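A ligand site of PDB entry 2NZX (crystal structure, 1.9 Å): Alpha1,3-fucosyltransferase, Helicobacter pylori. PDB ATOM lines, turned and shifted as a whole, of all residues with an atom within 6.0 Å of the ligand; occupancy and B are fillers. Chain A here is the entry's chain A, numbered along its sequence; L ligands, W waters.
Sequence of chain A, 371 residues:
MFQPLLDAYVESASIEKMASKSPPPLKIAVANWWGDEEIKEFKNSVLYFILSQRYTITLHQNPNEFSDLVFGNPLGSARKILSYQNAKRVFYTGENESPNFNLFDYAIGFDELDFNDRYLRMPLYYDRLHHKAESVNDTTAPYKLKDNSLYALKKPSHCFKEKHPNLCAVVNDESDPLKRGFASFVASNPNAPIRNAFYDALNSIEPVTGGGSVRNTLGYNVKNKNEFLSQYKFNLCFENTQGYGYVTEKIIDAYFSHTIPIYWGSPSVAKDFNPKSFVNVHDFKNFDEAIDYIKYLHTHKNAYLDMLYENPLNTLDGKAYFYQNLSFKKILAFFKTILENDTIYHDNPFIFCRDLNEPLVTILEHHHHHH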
ATOM      1  N   ARG A 128     -20.972 -40.255   9.712  1.00  0.00           N
ATOM      2  CA  ARG A 128     -21.025 -39.168   8.727  1.00  0.00           C
ATOM      3  C   ARG A 128     -21.095 -39.771   7.326  1.00  0.00           C
ATOM      4  O   ARG A 128     -21.810 -39.246   6.471  1.00  0.00           O
ATOM      5  CB  ARG A 128     -19.789 -38.242   8.806  1.00  0.00           C
ATOM      6  CG  ARG A 128     -19.967 -36.983   7.865  1.00  0.00           C
ATOM      7  CD  ARG A 128     -21.262 -36.288   8.235  1.00  0.00           C
ATOM      8  NE  ARG A 128     -21.130 -34.846   8.123  1.00  0.00           N
ATOM      9  CZ  ARG A 128     -21.672 -33.952   8.959  1.00  0.00           C
ATOM     10  NH1 ARG A 128     -22.434 -34.339   9.983  1.00  0.00           N
ATOM     11  NH2 ARG A 128     -21.376 -32.673   8.820  1.00  0.00           N
ATOM     12  N   VAL A 186     -14.471 -23.910   8.804  1.00  0.00           N
ATOM     13  CA  VAL A 186     -15.851 -23.822   9.268  1.00  0.00           C
ATOM     14  C   VAL A 186     -15.991 -24.332  10.685  1.00  0.00           C
ATOM     15  O   VAL A 186     -15.990 -25.556  10.932  1.00  0.00           O
ATOM     16  CB  VAL A 186     -16.813 -24.598   8.363  1.00  0.00           C
ATOM     17  CG1 VAL A 186     -18.259 -24.184   8.715  1.00  0.00           C
ATOM     18  CG2 VAL A 186     -16.504 -24.306   6.896  1.00  0.00           C
ATOM     19  N   ALA A 187     -16.117 -23.397  11.623  1.00  0.00           N
ATOM     20  CA  ALA A 187     -16.202 -23.740  13.033  1.00  0.00           C
ATOM     21  C   ALA A 187     -16.982 -22.697  13.814  1.00  0.00           C
ATOM     22  O   ALA A 187     -16.843 -21.497  13.567  1.00  0.00           O
ATOM     23  CB  ALA A 187     -14.772 -23.868  13.630  1.00  0.00           C
ATOM     24  N   SER A 188     -17.814 -23.162  14.734  1.00  0.00           N
ATOM     25  CA  SER A 188     -18.607 -22.281  15.581  1.00  0.00           C
ATOM     26  C   SER A 188     -18.336 -22.529  17.072  1.00  0.00           C
ATOM     27  O   SER A 188     -18.738 -21.739  17.926  1.00  0.00           O
ATOM     28  CB  SER A 188     -20.083 -22.416  15.252  1.00  0.00           C
ATOM     29  OG  SER A 188     -20.343 -21.878  13.952  1.00  0.00           O
ATOM     30  N   ASN A 189     -17.639 -23.616  17.376  1.00  0.00           N
ATOM     31  CA  ASN A 189     -17.258 -23.930  18.762  1.00  0.00           C
ATOM     32  C   ASN A 189     -15.923 -23.199  18.975  1.00  0.00           C
ATOM     33  O   ASN A 189     -14.865 -23.612  18.483  1.00  0.00           O
ATOM     34  CB  ASN A 189     -17.080 -25.450  18.918  1.00  0.00           C
ATOM     35  CG  ASN A 189     -16.388 -25.832  20.203  1.00  0.00           C
ATOM     36  OD1 ASN A 189     -16.485 -25.135  21.204  1.00  0.00           O
ATOM     37  ND2 ASN A 189     -15.687 -26.954  20.181  1.00  0.00           N
ATOM     38  N   PRO A 190     -15.969 -22.076  19.715  1.00  0.00           N
ATOM     39  CA  PRO A 190     -14.739 -21.298  19.963  1.00  0.00           C
ATOM     40  C   PRO A 190     -13.750 -21.959  20.925  1.00  0.00           C
ATOM     41  O   PRO A 190     -12.552 -21.750  20.847  1.00  0.00           O
ATOM     42  CB  PRO A 190     -15.285 -19.989  20.496  1.00  0.00           C
ATOM     43  CG  PRO A 190     -16.495 -20.469  21.313  1.00  0.00           C
ATOM     44  CD  PRO A 190     -17.130 -21.494  20.399  1.00  0.00           C
ATOM     45  N   ALA A 192     -11.670 -24.054  21.296  1.00  0.00           N
ATOM     46  CA  ALA A 192     -10.740 -24.957  20.616  1.00  0.00           C
ATOM     47  C   ALA A 192      -9.457 -24.199  20.315  1.00  0.00           C
ATOM     48  O   ALA A 192      -9.220 -23.793  19.180  1.00  0.00           O
ATOM     49  CB  ALA A 192     -11.372 -25.488  19.309  1.00  0.00           C
ATOM     50  N   ARG A 195      -6.886 -25.165  17.348  1.00  0.00           N
ATOM     51  CA  ARG A 195      -7.564 -24.925  16.079  1.00  0.00           C
ATOM     52  C   ARG A 195      -7.531 -23.435  15.722  1.00  0.00           C
ATOM     53  O   ARG A 195      -7.021 -23.035  14.677  1.00  0.00           O
ATOM     54  CB  ARG A 195      -9.002 -25.429  16.187  1.00  0.00           C
ATOM     55  CG  ARG A 195      -9.890 -25.173  15.020  1.00  0.00           C
ATOM     56  CD  ARG A 195     -11.025 -26.194  14.992  1.00  0.00           C
ATOM     57  NE  ARG A 195     -12.204 -25.841  15.765  1.00  0.00           N
ATOM     58  CZ  ARG A 195     -13.180 -26.696  16.034  1.00  0.00           C
ATOM     59  NH1 ARG A 195     -13.077 -27.938  15.575  1.00  0.00           N
ATOM     60  NH2 ARG A 195     -14.282 -26.325  16.709  1.00  0.00           N
ATOM     61  N   GLY A 211     -16.143 -19.620   7.439  1.00  0.00           N
ATOM     62  CA  GLY A 211     -17.571 -19.727   7.194  1.00  0.00           C
ATOM     63  C   GLY A 211     -18.440 -19.933   8.417  1.00  0.00           C
ATOM     64  O   GLY A 211     -19.654 -19.784   8.351  1.00  0.00           O
ATOM     65  N   GLY A 212     -17.829 -20.300   9.530  1.00  0.00           N
ATOM     66  CA  GLY A 212     -18.580 -20.486  10.764  1.00  0.00           C
ATOM     67  C   GLY A 212     -18.495 -19.236  11.644  1.00  0.00           C
ATOM     68  O   GLY A 212     -17.967 -18.206  11.200  1.00  0.00           O
ATOM     69  N   SER A 213     -19.011 -19.306  12.871  1.00  0.00           N
ATOM     70  CA  SER A 213     -18.971 -18.159  13.777  1.00  0.00           C
ATOM     71  C   SER A 213     -17.529 -17.804  14.211  1.00  0.00           C
ATOM     72  O   SER A 213     -17.241 -16.651  14.548  1.00  0.00           O
ATOM     73  CB  SER A 213     -19.865 -18.411  15.015  1.00  0.00           C
ATOM     74  OG  SER A 213     -19.345 -19.432  15.878  1.00  0.00           O
ATOM     75  N   ASN A 221     -22.962 -16.903   8.474  1.00  0.00           N
ATOM     76  CA  ASN A 221     -22.657 -18.332   8.646  1.00  0.00           C
ATOM     77  C   ASN A 221     -23.158 -19.161   7.483  1.00  0.00           C
ATOM     78  O   ASN A 221     -24.362 -19.242   7.229  1.00  0.00           O
ATOM     79  CB  ASN A 221     -23.277 -18.858   9.943  1.00  0.00           C
ATOM     80  CG  ASN A 221     -22.544 -18.369  11.171  1.00  0.00           C
ATOM     81  OD1 ASN A 221     -23.071 -18.441  12.299  1.00  0.00           O
ATOM     82  ND2 ASN A 221     -21.331 -17.874  10.976  1.00  0.00           N
ATOM     83  N   VAL A 222     -22.221 -19.812   6.791  1.00  0.00           N
ATOM     84  CA  VAL A 222     -22.536 -20.640   5.634  1.00  0.00           C
ATOM     85  C   VAL A 222     -23.601 -21.682   5.952  1.00  0.00           C
ATOM     86  O   VAL A 222     -23.538 -22.367   6.985  1.00  0.00           O
ATOM     87  CB  VAL A 222     -21.256 -21.317   5.091  1.00  0.00           C
ATOM     88  CG1 VAL A 222     -20.851 -22.494   5.987  1.00  0.00           C
ATOM     89  CG2 VAL A 222     -21.449 -21.710   3.649  1.00  0.00           C
ATOM     90  N   LYS A 223     -24.568 -21.787   5.048  1.00  0.00           N
ATOM     91  CA  LYS A 223     -25.681 -22.707   5.184  1.00  0.00           C
ATOM     92  C   LYS A 223     -25.328 -24.129   4.782  1.00  0.00           C
ATOM     93  O   LYS A 223     -25.643 -25.080   5.522  1.00  0.00           O
ATOM     94  CB  LYS A 223     -26.851 -22.181   4.355  1.00  0.00           C
ATOM     95  CG  LYS A 223     -28.168 -22.777   4.697  1.00  0.00           C
ATOM     96  CD  LYS A 223     -28.417 -24.056   3.926  1.00  0.00           C
ATOM     97  CE  LYS A 223     -29.927 -24.370   3.883  1.00  0.00           C
ATOM     98  NZ  LYS A 223     -30.682 -23.370   3.059  1.00  0.00           N
ATOM     99  N   ASN A 224     -24.698 -24.306   3.623  1.00  0.00           N
ATOM    100  CA  ASN A 224     -24.286 -25.654   3.291  1.00  0.00           C
ATOM    101  C   ASN A 224     -22.787 -25.760   3.367  1.00  0.00           C
ATOM    102  O   ASN A 224     -22.041 -25.245   2.523  1.00  0.00           O
ATOM    103  CB  ASN A 224     -24.693 -26.158   1.911  1.00  0.00           C
ATOM    104  CG  ASN A 224     -24.105 -27.561   1.679  1.00  0.00           C
ATOM    105  OD1 ASN A 224     -23.179 -27.738   0.886  1.00  0.00           O
ATOM    106  ND2 ASN A 224     -24.603 -28.552   2.424  1.00  0.00           N
ATOM    107  N   LYS A 225     -22.335 -26.434   4.409  1.00  0.00           N
ATOM    108  CA  LYS A 225     -20.897 -26.584   4.563  1.00  0.00           C
ATOM    109  C   LYS A 225     -20.261 -27.256   3.351  1.00  0.00           C
ATOM    110  O   LYS A 225     -19.236 -26.786   2.830  1.00  0.00           O
ATOM    111  CB  LYS A 225     -20.541 -27.386   5.856  1.00  0.00           C
ATOM    112  CG  LYS A 225     -19.041 -27.752   5.965  1.00  0.00           C
ATOM    113  CD  LYS A 225     -18.738 -28.552   7.228  1.00  0.00           C
ATOM    114  CE  LYS A 225     -17.223 -28.857   7.348  1.00  0.00           C
ATOM    115  NZ  LYS A 225     -16.807 -29.911   8.407  1.00  0.00           N
ATOM    116  N   PHE A 238      -9.660 -29.386  11.676  1.00  0.00           N
ATOM    117  CA  PHE A 238      -9.153 -29.733  13.001  1.00  0.00           C
ATOM    118  C   PHE A 238     -10.255 -30.154  13.955  1.00  0.00           C
ATOM    119  O   PHE A 238     -11.305 -29.510  14.001  1.00  0.00           O
ATOM    120  CB  PHE A 238      -8.502 -28.505  13.636  1.00  0.00           C
ATOM    121  CG  PHE A 238      -7.086 -28.275  13.220  1.00  0.00           C
ATOM    122  CD1 PHE A 238      -6.668 -28.521  11.909  1.00  0.00           C
ATOM    123  CD2 PHE A 238      -6.163 -27.777  14.144  1.00  0.00           C
ATOM    124  CE1 PHE A 238      -5.333 -28.269  11.514  1.00  0.00           C
ATOM    125  CE2 PHE A 238      -4.833 -27.522  13.772  1.00  0.00           C
ATOM    126  CZ  PHE A 238      -4.420 -27.766  12.468  1.00  0.00           C
ATOM    127  N   GLU A 239      -9.991 -31.210  14.738  1.00  0.00           N
ATOM    128  CA  GLU A 239     -10.952 -31.656  15.772  1.00  0.00           C
ATOM    129  C   GLU A 239     -10.885 -30.567  16.868  1.00  0.00           C
ATOM    130  O   GLU A 239      -9.981 -29.736  16.884  1.00  0.00           O
ATOM    131  CB  GLU A 239     -10.514 -33.002  16.355  1.00  0.00           C
ATOM    132  CG  GLU A 239     -10.282 -34.102  15.332  1.00  0.00           C
ATOM    133  CD  GLU A 239     -11.529 -34.567  14.622  1.00  0.00           C
ATOM    134  OE1 GLU A 239     -12.638 -34.042  14.855  1.00  0.00           O
ATOM    135  OE2 GLU A 239     -11.401 -35.464  13.808  1.00  0.00           O
ATOM    136  N   ASN A 240     -11.844 -30.550  17.801  1.00  0.00           N
ATOM    137  CA  ASN A 240     -11.822 -29.555  18.843  1.00  0.00           C
ATOM    138  C   ASN A 240     -10.831 -29.912  19.945  1.00  0.00           C
ATOM    139  O   ASN A 240     -10.455 -29.063  20.718  1.00  0.00           O
ATOM    140  CB  ASN A 240     -13.218 -29.366  19.440  1.00  0.00           C
ATOM    141  CG  ASN A 240     -13.825 -30.668  19.986  1.00  0.00           C
ATOM    142  OD1 ASN A 240     -13.122 -31.551  20.522  1.00  0.00           O
ATOM    143  ND2 ASN A 240     -15.123 -30.796  19.836  1.00  0.00           N
ATOM    144  N   TYR A 246      -9.816 -40.322  17.969  1.00  0.00           N
ATOM    145  CA  TYR A 246     -10.928 -39.382  17.899  1.00  0.00           C
ATOM    146  C   TYR A 246     -11.025 -38.688  16.538  1.00  0.00           C
ATOM    147  O   TYR A 246     -10.577 -37.550  16.369  1.00  0.00           O
ATOM    148  CB  TYR A 246     -10.807 -38.364  19.041  1.00  0.00           C
ATOM    149  CG  TYR A 246     -12.028 -37.487  19.171  1.00  0.00           C
ATOM    150  CD1 TYR A 246     -13.290 -38.062  19.332  1.00  0.00           C
ATOM    151  CD2 TYR A 246     -11.939 -36.085  19.098  1.00  0.00           C
ATOM    152  CE1 TYR A 246     -14.432 -37.279  19.428  1.00  0.00           C
ATOM    153  CE2 TYR A 246     -13.102 -35.290  19.189  1.00  0.00           C
ATOM    154  CZ  TYR A 246     -14.316 -35.891  19.354  1.00  0.00           C
ATOM    155  OH  TYR A 246     -15.465 -35.151  19.572  1.00  0.00           O
ATOM    156  N   THR A 248     -13.702 -37.439  13.855  1.00  0.00           N
ATOM    157  CA  THR A 248     -15.105 -37.155  13.673  1.00  0.00           C
ATOM    158  C   THR A 248     -15.568 -37.002  12.231  1.00  0.00           C
ATOM    159  O   THR A 248     -14.936 -37.541  11.310  1.00  0.00           O
ATOM    160  CB  THR A 248     -15.519 -35.952  14.490  1.00  0.00           C
ATOM    161  OG1 THR A 248     -14.900 -34.759  13.977  1.00  0.00           O
ATOM    162  CG2 THR A 248     -15.050 -36.143  15.957  1.00  0.00           C
ATOM    163  N   GLU A 249     -16.685 -36.300  12.055  1.00  0.00           N
ATOM    164  CA  GLU A 249     -17.252 -36.142  10.711  1.00  0.00           C
ATOM    165  C   GLU A 249     -16.419 -35.139   9.866  1.00  0.00           C
ATOM    166  O   GLU A 249     -16.469 -35.149   8.661  1.00  0.00           O
ATOM    167  CB  GLU A 249     -18.699 -35.650  10.824  1.00  0.00           C
ATOM    168  CG  GLU A 249     -18.842 -34.173  11.121  1.00  0.00           C
ATOM    169  CD  GLU A 249     -18.375 -33.741  12.539  1.00  0.00           C
ATOM    170  OE1 GLU A 249     -18.258 -34.625  13.426  1.00  0.00           O
ATOM    171  OE2 GLU A 249     -18.146 -32.514  12.773  1.00  0.00           O
ATOM    172  N   LYS A 250     -15.628 -34.309  10.520  1.00  0.00           N
ATOM    173  CA  LYS A 250     -14.881 -33.300   9.800  1.00  0.00           C
ATOM    174  C   LYS A 250     -14.112 -33.753   8.580  1.00  0.00           C
ATOM    175  O   LYS A 250     -14.374 -33.247   7.493  1.00  0.00           O
ATOM    176  CB  LYS A 250     -13.980 -32.558  10.782  1.00  0.00           C
ATOM    177  CG  LYS A 250     -14.808 -31.928  11.916  1.00  0.00           C
ATOM    178  CD  LYS A 250     -13.918 -31.392  13.090  1.00  0.00           C
ATOM    179  CE  LYS A 250     -14.804 -30.879  14.216  1.00  0.00           C
ATOM    180  NZ  LYS A 250     -15.821 -31.903  14.698  1.00  0.00           N
ATOM    181  N   ASP A 253     -16.212 -34.605   5.604  1.00  0.00           N
ATOM    182  CA  ASP A 253     -16.744 -33.425   4.930  1.00  0.00           C
ATOM    183  C   ASP A 253     -15.736 -32.892   3.902  1.00  0.00           C
ATOM    184  O   ASP A 253     -16.118 -32.434   2.820  1.00  0.00           O
ATOM    185  CB  ASP A 253     -17.089 -32.382   5.968  1.00  0.00           C
ATOM    186  CG  ASP A 253     -18.382 -32.703   6.696  1.00  0.00           C
ATOM    187  OD1 ASP A 253     -19.164 -33.568   6.239  1.00  0.00           O
ATOM    188  OD2 ASP A 253     -18.621 -32.070   7.714  1.00  0.00           O
HETATM  189  P1  LIG L   1     -16.957 -28.835  17.004  1.00  0.00           P
HETATM  190  O1  LIG L   1     -16.294 -28.667  18.274  1.00  0.00           O
HETATM  191  O2  LIG L   1     -17.241 -30.409  16.777  1.00  0.00           O
HETATM  192  O3  LIG L   1     -15.994 -28.246  15.902  1.00  0.00           O
HETATM  193  O4  LIG L   1     -18.424 -28.111  17.011  1.00  0.00           O
HETATM  194  P2  LIG L   1     -18.673 -26.991  15.823  1.00  0.00           P
HETATM  195  O5  LIG L   1     -19.912 -26.259  16.139  1.00  0.00           O
HETATM  196  O6  LIG L   1     -17.476 -25.951  15.741  1.00  0.00           O
HETATM  197  O7  LIG L   1     -18.860 -27.629  14.376  1.00  0.00           O
HETATM  198  C1  LIG L   1     -19.513 -28.874  14.418  1.00  0.00           C
HETATM  199  C2  LIG L   1     -19.783 -29.276  12.929  1.00  0.00           C
HETATM  200  O8  LIG L   1     -20.672 -28.315  12.305  1.00  0.00           O
HETATM  201  C3  LIG L   1     -18.504 -29.264  12.077  1.00  0.00           C
HETATM  202  O9  LIG L   1     -18.536 -30.236  11.048  1.00  0.00           O
HETATM  203  C4  LIG L   1     -18.476 -27.883  11.519  1.00  0.00           C
HETATM  204  O10 LIG L   1     -17.631 -27.826  10.376  1.00  0.00           O
HETATM  205  C5  LIG L   1     -19.957 -27.624  11.242  1.00  0.00           C
HETATM  206  N1  LIG L   1     -20.245 -26.212  11.321  1.00  0.00           N
HETATM  207  C6  LIG L   1     -19.769 -25.349  12.275  1.00  0.00           C
HETATM  208  N2  LIG L   1     -20.202 -24.158  12.041  1.00  0.00           N
HETATM  209  C7  LIG L   1     -20.987 -24.178  10.939  1.00  0.00           C
HETATM  210  C8  LIG L   1     -21.711 -23.178  10.205  1.00  0.00           C
HETATM  211  O11 LIG L   1     -21.706 -21.978  10.591  1.00  0.00           O
HETATM  212  N3  LIG L   1     -22.432 -23.594   9.074  1.00  0.00           N
HETATM  213  C9  LIG L   1     -22.420 -24.939   8.682  1.00  0.00           C
HETATM  214  N4  LIG L   1     -23.129 -25.342   7.584  1.00  0.00           N
HETATM  215  N5  LIG L   1     -21.732 -25.840   9.365  1.00  0.00           N
HETATM  216  C10 LIG L   1     -21.017 -25.508  10.472  1.00  0.00           C
HETATM  217  O   HOH W   1     -14.341 -28.744   9.685  1.00  0.00           O
HETATM  218  O   HOH W   2     -19.947 -31.730  17.135  1.00  0.00           O
HETATM  219  O   HOH W   3     -20.883 -30.498   9.871  1.00  0.00           O
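The side-chain carboxylate of Glu 239 is in salt-bridge range of the side-chain amino group of Lys 250 (3.8 Å). The side-chain amide nitrogen of Asn 221 sits close to the backbone carbonyl oxygen of Gly 212 (3.4 Å). The side-chain carboxylate (OE1) of Glu 249 lies close to the side-chain hydroxyl (OG1) of Thr 248, 3.4 Å away. The backbone carbonyl oxygen (O) of Asn 189 is in hydrogen-bond range of the guanidinium group (NH2) of Arg 195 (3.3 Å). The side-chain amide nitrogen (ND2) of Asn 221 sits close to the backbone NH (N) of Ser 213, at 3.3 Å. The backbone carbonyl oxygen (O) of Ala 187 lies within hydrogen-bond range of the backbone NH (N) of Ser 213, at 3.2 Å. OE2 of Glu 249 lies within salt-bridge range of NZ of Lys 250 (3.1 Å). The side-chain amino group (NZ) of Lys 250 is in hydrogen-bond range of the side-chain hydroxyl (OG1) of Thr 248 (3.1 Å).
Water W3 lies within hydrogen-bond range of the guanidinium group (NH2) of Arg 128 (2.5 Å), an oxygen (O9) of the ligand (2.6 Å) and the side-chain carboxylate (OD2) of Asp 253 (3.5 Å). Water W1 bridges the side-chain amino group (NZ) of Lys 225 (3.0 Å) and an oxygen (O10) of the ligand (3.5 Å).
Residues that only touch the ligand: Gly 212 (3.5 Å), Asn 221 (3.6 Å), Ala 187 (3.7 Å), Gly 211 (3.7 Å) and Asp 253 (3.8 Å). Hydrophobic or aromatic side chains within 4 Å of the ligand: Val 186 and Val 222. Of the 24 residues printed, 15 come within 4 Å of the ligand.
The side-chain amide nitrogen (ND2) of Asn 189 is in hydrogen-bond range of an oxygen (O1) of the ligand, 2.6 Å away. NZ of Lys 225 lies within hydrogen-bond range of O10 of the ligand (3.0 Å). An oxygen (O2) of the ligand lies within salt-bridge range of the side-chain amino group (NZ) of Lys 250 (2.9 Å). An oxygen (O6) of the ligand lies within hydrogen-bond range of the backbone NH (N) of Asn 189, at 2.9 Å. O of Val 222 is in hydrogen-bond range of N3 of the ligand, at 2.7 Å. The side-chain amide nitrogen (ND2) of Asn 240 sits at hydrogen-bond distance from an oxygen (O1) of the ligand (2.9 Å). An oxygen (O3) of the ligand lies within salt-bridge range of the guanidinium group (NH2) of Arg 195 (2.7 Å). The side-chain hydroxyl (OG) of Ser 188 is in hydrogen-bond range of a nitrogen (N2) of the ligand (3.0 Å). N4 of the ligand sits at hydrogen-bond distance from O of Lys 223, at 3.3 Å. The backbone carbonyl oxygen (O) of Val 186 is in hydrogen-bond range of an oxygen (O10) of the ligand, at 2.9 Å. N of Ser 188 sits at hydrogen-bond distance from O6 of the ligand (3.0 Å). OE2 of Glu 249 is in hydrogen-bond range of O9 of the ligand (2.9 Å).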
